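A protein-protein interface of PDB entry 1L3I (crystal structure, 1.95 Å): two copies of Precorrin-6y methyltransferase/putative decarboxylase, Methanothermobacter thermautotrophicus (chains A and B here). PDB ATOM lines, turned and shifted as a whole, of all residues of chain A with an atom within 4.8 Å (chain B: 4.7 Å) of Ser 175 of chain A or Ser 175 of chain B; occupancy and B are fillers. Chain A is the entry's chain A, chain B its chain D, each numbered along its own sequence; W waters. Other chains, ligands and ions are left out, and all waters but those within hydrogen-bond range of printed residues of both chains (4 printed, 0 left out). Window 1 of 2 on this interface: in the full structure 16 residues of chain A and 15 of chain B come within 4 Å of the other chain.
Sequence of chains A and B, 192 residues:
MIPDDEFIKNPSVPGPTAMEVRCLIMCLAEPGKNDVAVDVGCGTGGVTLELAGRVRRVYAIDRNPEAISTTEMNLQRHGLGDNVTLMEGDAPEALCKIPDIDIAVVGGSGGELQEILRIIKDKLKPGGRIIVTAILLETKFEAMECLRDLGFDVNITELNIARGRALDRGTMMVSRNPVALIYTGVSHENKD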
ATOM      1  N   ASN A 160      17.981  17.917 -20.427  1.00  0.00           N
ATOM      2  CA  ASN A 160      18.553  18.775 -21.449  1.00  0.00           C
ATOM      3  C   ASN A 160      20.046  18.533 -21.286  1.00  0.00           C
ATOM      4  O   ASN A 160      20.628  18.889 -20.252  1.00  0.00           O
ATOM      5  CB  ASN A 160      18.196  20.235 -21.230  1.00  0.00           C
ATOM      6  CG  ASN A 160      16.928  20.640 -21.973  1.00  0.00           C
ATOM      7  OD1 ASN A 160      16.946  20.900 -23.185  1.00  0.00           O
ATOM      8  ND2 ASN A 160      15.822  20.682 -21.252  1.00  0.00           N
ATOM      9  N   ILE A 161      20.624  17.819 -22.252  1.00  0.00           N
ATOM     10  CA  ILE A 161      22.042  17.461 -22.217  1.00  0.00           C
ATOM     11  C   ILE A 161      22.875  18.241 -23.211  1.00  0.00           C
ATOM     12  O   ILE A 161      22.466  18.447 -24.350  1.00  0.00           O
ATOM     13  CB  ILE A 161      22.232  15.965 -22.520  1.00  0.00           C
ATOM     14  CG1 ILE A 161      21.376  15.139 -21.580  1.00  0.00           C
ATOM     15  CG2 ILE A 161      23.695  15.583 -22.396  1.00  0.00           C
ATOM     16  CD1 ILE A 161      20.878  13.864 -22.225  1.00  0.00           C
ATOM     17  N   ALA A 162      24.059  18.655 -22.769  1.00  0.00           N
ATOM     18  CA  ALA A 162      24.995  19.383 -23.603  1.00  0.00           C
ATOM     19  C   ALA A 162      26.339  18.698 -23.416  1.00  0.00           C
ATOM     20  O   ALA A 162      26.695  18.306 -22.300  1.00  0.00           O
ATOM     21  CB  ALA A 162      25.082  20.843 -23.196  1.00  0.00           C
ATOM     22  N   MET A 173      29.756  24.077 -26.315  1.00  0.00           N
ATOM     23  CA  MET A 173      28.800  23.130 -25.798  1.00  0.00           C
ATOM     24  C   MET A 173      27.745  22.833 -26.867  1.00  0.00           C
ATOM     25  O   MET A 173      27.135  23.746 -27.428  1.00  0.00           O
ATOM     26  CB  MET A 173      28.169  23.689 -24.518  1.00  0.00           C
ATOM     27  CG  MET A 173      29.168  24.000 -23.413  1.00  0.00           C
ATOM     28  SD  MET A 173      30.232  22.478 -22.847  1.00  0.00           S
ATOM     29  CE  MET A 173      28.841  21.244 -22.335  1.00  0.00           C
ATOM     30  N   VAL A 174      27.572  21.549 -27.175  1.00  0.00           N
ATOM     31  CA  VAL A 174      26.601  21.116 -28.175  1.00  0.00           C
ATOM     32  C   VAL A 174      25.426  20.436 -27.478  1.00  0.00           C
ATOM     33  O   VAL A 174      25.609  19.423 -26.808  1.00  0.00           O
ATOM     34  CB  VAL A 174      27.249  20.130 -29.177  1.00  0.00           C
ATOM     35  CG1 VAL A 174      26.218  19.658 -30.183  1.00  0.00           C
ATOM     36  CG2 VAL A 174      28.425  20.810 -29.907  1.00  0.00           C
ATOM     37  N   SER A 175      24.230  20.993 -27.628  1.00  0.00           N
ATOM     38  CA  SER A 175      23.051  20.428 -26.983  1.00  0.00           C
ATOM     39  C   SER A 175      22.366  19.320 -27.782  1.00  0.00           C
ATOM     40  O   SER A 175      22.499  19.224 -28.996  1.00  0.00           O
ATOM     41  CB  SER A 175      22.035  21.527 -26.706  1.00  0.00           C
ATOM     42  OG  SER A 175      21.639  22.136 -27.923  1.00  0.00           O
ATOM     43  N   ARG A 176      21.651  18.469 -27.071  1.00  0.00           N
ATOM     44  CA  ARG A 176      20.897  17.391 -27.690  1.00  0.00           C
ATOM     45  C   ARG A 176      19.466  17.800 -27.458  1.00  0.00           C
ATOM     46  O   ARG A 176      19.181  18.533 -26.502  1.00  0.00           O
ATOM     47  CB  ARG A 176      21.142  16.062 -26.978  1.00  0.00           C
ATOM     48  CG  ARG A 176      22.580  15.649 -26.965  1.00  0.00           C
ATOM     49  CD  ARG A 176      22.724  14.336 -26.275  1.00  0.00           C
ATOM     50  NE  ARG A 176      23.991  13.703 -26.629  1.00  0.00           N
ATOM     51  CZ  ARG A 176      24.215  12.391 -26.570  1.00  0.00           C
ATOM     52  NH1 ARG A 176      23.272  11.572 -26.181  1.00  0.00           N
ATOM     53  NH2 ARG A 176      25.343  11.877 -27.014  1.00  0.00           N
ATOM     54  N   ASN A 177      18.568  17.374 -28.337  1.00  0.00           N
ATOM     55  CA  ASN A 177      17.161  17.711 -28.180  1.00  0.00           C
ATOM     56  C   ASN A 177      16.673  17.166 -26.840  1.00  0.00           C
ATOM     57  O   ASN A 177      17.109  16.105 -26.401  1.00  0.00           O
ATOM     58  CB  ASN A 177      16.326  17.119 -29.318  1.00  0.00           C
ATOM     59  CG  ASN A 177      16.679  17.722 -30.665  1.00  0.00           C
ATOM     60  OD1 ASN A 177      17.022  18.897 -30.770  1.00  0.00           O
ATOM     61  ND2 ASN A 177      16.609  16.908 -31.702  1.00  0.00           N
ATOM     62  N   PRO A 178      15.824  17.929 -26.142  1.00  0.00           N
ATOM     63  CA  PRO A 178      15.338  17.430 -24.862  1.00  0.00           C
ATOM     64  C   PRO A 178      14.530  16.148 -24.998  1.00  0.00           C
ATOM     65  O   PRO A 178      13.872  15.922 -26.002  1.00  0.00           O
ATOM     66  CB  PRO A 178      14.498  18.606 -24.344  1.00  0.00           C
ATOM     67  CG  PRO A 178      14.069  19.307 -25.552  1.00  0.00           C
ATOM     68  CD  PRO A 178      15.306  19.278 -26.409  1.00  0.00           C
ATOM     69  N   ILE B 161      17.732  27.136 -25.232  1.00  0.00           N
ATOM     70  CA  ILE B 161      16.481  27.321 -25.974  1.00  0.00           C
ATOM     71  C   ILE B 161      16.070  26.097 -26.778  1.00  0.00           C
ATOM     72  O   ILE B 161      16.899  25.431 -27.412  1.00  0.00           O
ATOM     73  CB  ILE B 161      16.599  28.510 -26.958  1.00  0.00           C
ATOM     74  CG1 ILE B 161      17.052  29.757 -26.201  1.00  0.00           C
ATOM     75  CG2 ILE B 161      15.268  28.753 -27.670  1.00  0.00           C
ATOM     76  CD1 ILE B 161      17.910  30.653 -27.049  1.00  0.00           C
ATOM     77  N   ALA B 162      14.773  25.816 -26.759  1.00  0.00           N
ATOM     78  CA  ALA B 162      14.219  24.691 -27.499  1.00  0.00           C
ATOM     79  C   ALA B 162      13.008  25.238 -28.241  1.00  0.00           C
ATOM     80  O   ALA B 162      12.241  26.023 -27.692  1.00  0.00           O
ATOM     81  CB  ALA B 162      13.819  23.559 -26.561  1.00  0.00           C
ATOM     82  N   MET B 173      10.568  18.920 -29.729  1.00  0.00           N
ATOM     83  CA  MET B 173      11.326  20.051 -29.214  1.00  0.00           C
ATOM     84  C   MET B 173      12.752  19.975 -29.731  1.00  0.00           C
ATOM     85  O   MET B 173      13.419  18.945 -29.576  1.00  0.00           O
ATOM     86  CB  MET B 173      11.299  20.051 -27.683  1.00  0.00           C
ATOM     87  CG  MET B 173       9.899  20.228 -27.073  1.00  0.00           C
ATOM     88  SD  MET B 173       8.911  21.761 -27.760  1.00  0.00           S
ATOM     89  CE  MET B 173       9.959  23.244 -27.107  1.00  0.00           C
ATOM     90  N   VAL B 174      13.200  21.030 -30.411  1.00  0.00           N
ATOM     91  CA  VAL B 174      14.550  21.041 -30.962  1.00  0.00           C
ATOM     92  C   VAL B 174      15.370  22.050 -30.207  1.00  0.00           C
ATOM     93  O   VAL B 174      15.004  23.224 -30.127  1.00  0.00           O
ATOM     94  CB  VAL B 174      14.562  21.381 -32.474  1.00  0.00           C
ATOM     95  CG1 VAL B 174      15.952  21.222 -33.025  1.00  0.00           C
ATOM     96  CG2 VAL B 174      13.605  20.469 -33.221  1.00  0.00           C
ATOM     97  N   SER B 175      16.467  21.598 -29.626  1.00  0.00           N
ATOM     98  CA  SER B 175      17.324  22.489 -28.863  1.00  0.00           C
ATOM     99  C   SER B 175      18.382  23.196 -29.697  1.00  0.00           C
ATOM    100  O   SER B 175      18.766  22.743 -30.775  1.00  0.00           O
ATOM    101  CB  SER B 175      18.013  21.720 -27.733  1.00  0.00           C
ATOM    102  OG  SER B 175      18.855  20.703 -28.257  1.00  0.00           O
ATOM    103  N   ARG B 176      18.820  24.338 -29.193  1.00  0.00           N
ATOM    104  CA  ARG B 176      19.867  25.117 -29.813  1.00  0.00           C
ATOM    105  C   ARG B 176      21.008  25.005 -28.837  1.00  0.00           C
ATOM    106  O   ARG B 176      20.771  24.809 -27.639  1.00  0.00           O
ATOM    107  CB  ARG B 176      19.463  26.578 -29.912  1.00  0.00           C
ATOM    108  CG  ARG B 176      18.242  26.807 -30.744  1.00  0.00           C
ATOM    109  CD  ARG B 176      17.947  28.266 -30.839  1.00  0.00           C
ATOM    110  NE  ARG B 176      17.031  28.537 -31.940  1.00  0.00           N
ATOM    111  CZ  ARG B 176      16.930  29.710 -32.557  1.00  0.00           C
ATOM    112  NH1 ARG B 176      17.681  30.719 -32.188  1.00  0.00           N
ATOM    113  NH2 ARG B 176      16.159  29.848 -33.609  1.00  0.00           N
ATOM    114  N   ASN B 177      22.244  25.081 -29.325  1.00  0.00           N
ATOM    115  CA  ASN B 177      23.398  25.007 -28.437  1.00  0.00           C
ATOM    116  C   ASN B 177      23.303  26.135 -27.411  1.00  0.00           C
ATOM    117  O   ASN B 177      22.832  27.225 -27.716  1.00  0.00           O
ATOM    118  CB  ASN B 177      24.691  25.127 -29.236  1.00  0.00           C
ATOM    119  CG  ASN B 177      24.877  23.980 -30.190  1.00  0.00           C
ATOM    120  OD1 ASN B 177      24.464  22.851 -29.920  1.00  0.00           O
ATOM    121  ND2 ASN B 177      25.476  24.262 -31.332  1.00  0.00           N
ATOM    122  N   PRO B 178      23.696  25.862 -26.170  1.00  0.00           N
ATOM    123  CA  PRO B 178      23.620  26.914 -25.168  1.00  0.00           C
ATOM    124  C   PRO B 178      24.545  28.093 -25.464  1.00  0.00           C
ATOM    125  O   PRO B 178      25.621  27.929 -26.031  1.00  0.00           O
ATOM    126  CB  PRO B 178      24.020  26.182 -23.891  1.00  0.00           C
ATOM    127  CG  PRO B 178      24.865  25.081 -24.353  1.00  0.00           C
ATOM    128  CD  PRO B 178      24.171  24.603 -25.585  1.00  0.00           C
HETATM  129  O   HOH W   1      27.251  26.620 -27.984  1.00  0.00           O
HETATM  130  O   HOH W   2      19.374  19.781 -31.720  1.00  0.00           O
HETATM  131  O   HOH W   3      22.865  21.208 -31.321  1.00  0.00           O
HETATM  132  O   HOH W   4      13.198  16.086 -28.940  1.00  0.00           O
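The backbone NH (N) of Ser 175 of chain A is in hydrogen-bond range of the side-chain amide oxygen (OD1) of Asn 177 of chain B, 3.0 Å away.
The side-chain hydroxyl (OG) of Ser 175 of chain A lies within hydrogen-bond range of the side-chain hydroxyl (OG) of Ser 175 of chain B, 3.1 Å away.
N of Ser 175 of chain B sits at hydrogen-bond distance from OD1 of Asn 177 of chain A (3.0 Å).
OG of Ser 175 of chain A sits at hydrogen-bond distance from O of Arg 176 of chain B (2.8 Å).
O of Arg 176 of chain A lies within hydrogen-bond range of OG of Ser 175 of chain B, 2.8 Å away.
The backbone NH of Arg 176 of chain B sits at hydrogen-bond distance from the backbone carbonyl oxygen of Ile 161 of chain B (2.8 Å).
The backbone carbonyl oxygen of Ile 161 of chain A sits at hydrogen-bond distance from the backbone NH of Arg 176 of chain A (2.8 Å).
Among the printed residues, pairs that only touch across the chains: Met 173 of chain A with Asn 177 of chain B (3.3 Å), Met 173 of chain A with Pro 178 of chain B (3.6 Å), Val 174 of chain A with Asn 177 of chain B (3.3 Å), Ser 175 of chain A with Pro 178 of chain B (3.9 Å), Asn 177 of chain A with Met 173 of chain B (3.4 Å), Asn 177 of chain A with Val 174 of chain B (3.3 Å), Pro 178 of chain A with Met 173 of chain B (3.6 Å) and Pro 178 of chain A with Ser 175 of chain B (3.9 Å).
Ala 162 of chain A touches none of the printed residues of chain B.
Printed residues of chain B within 4 Å of Ser 175 of chain A: Ser 175, Arg 176, Asn 177 and Pro 178.
Printed residues of chain B within 4 Å of Arg 176 of chain A: Ser 175 (2.8 Å).
Of the printed residues of chain B, Asn 177 of chain A touches Met 173 (3.4 Å), Val 174 (3.3 Å) and Ser 175 (3.0 Å).
Ala 162 of chain B touches none of the printed residues of chain A.
Printed residues of chain A within 4 Å of Ser 175 of chain B: Ser 175, Arg 176, Asn 177 and Pro 178.
Of the printed residues of chain A, Asn 177 of chain B touches Met 173 (3.3 Å), Val 174 (3.3 Å) and Ser 175 (3.0 Å).
The nearest residue of chain A that does not touch Ser 175 of chain B is Asn 160 of chain A (4.7 Å).
Hydrophobic or aromatic side chains of chain B within 4 Å of the printed part of chain A: Met 173, Val 174 and Pro 178.
Among the printed residues, 13 pairs touch across the chains.
Among the printed residues, no Asp or Glu carboxylate lies within 4 Å of a Lys or Arg side-chain nitrogen of the other chain.
Met 173 of chain A touches Asn 177 of chain B, and with the chains exchanged Asn 177 of chain A touches Met 173 of chain B.
Met 173 of chain A touches Pro 178 of chain B, and with the chains exchanged Pro 178 of chain A touches Met 173 of chain B.
Ser 175 of chain A touches its own counterpart, Ser 175 of chain B.
Ser 175 of chain A touches Asn 177 of chain B, and with the chains exchanged Asn 177 of chain A touches Ser 175 of chain B.
Water W2 lies within hydrogen-bond range of OD1 of Asn 177 of chain A (2.7 Å) and O of Ser 175 of chain B (3.2 Å).
Water W3 lies within hydrogen-bond range of the side-chain amide oxygen (OD1) of Asn 177 of chain B (2.7 Å) and the backbone carbonyl oxygen (O) of Ser 175 of chain A (3.1 Å).
Water W1 bridges the backbone carbonyl oxygen of Pro 178 of chain B (2.9 Å) and the backbone carbonyl oxygen of Met 173 of chain A (2.9 Å).
Water W4 lies within hydrogen-bond range of O of Met 173 of chain B (2.9 Å) and O of Pro 178 of chain A (3.0 Å).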
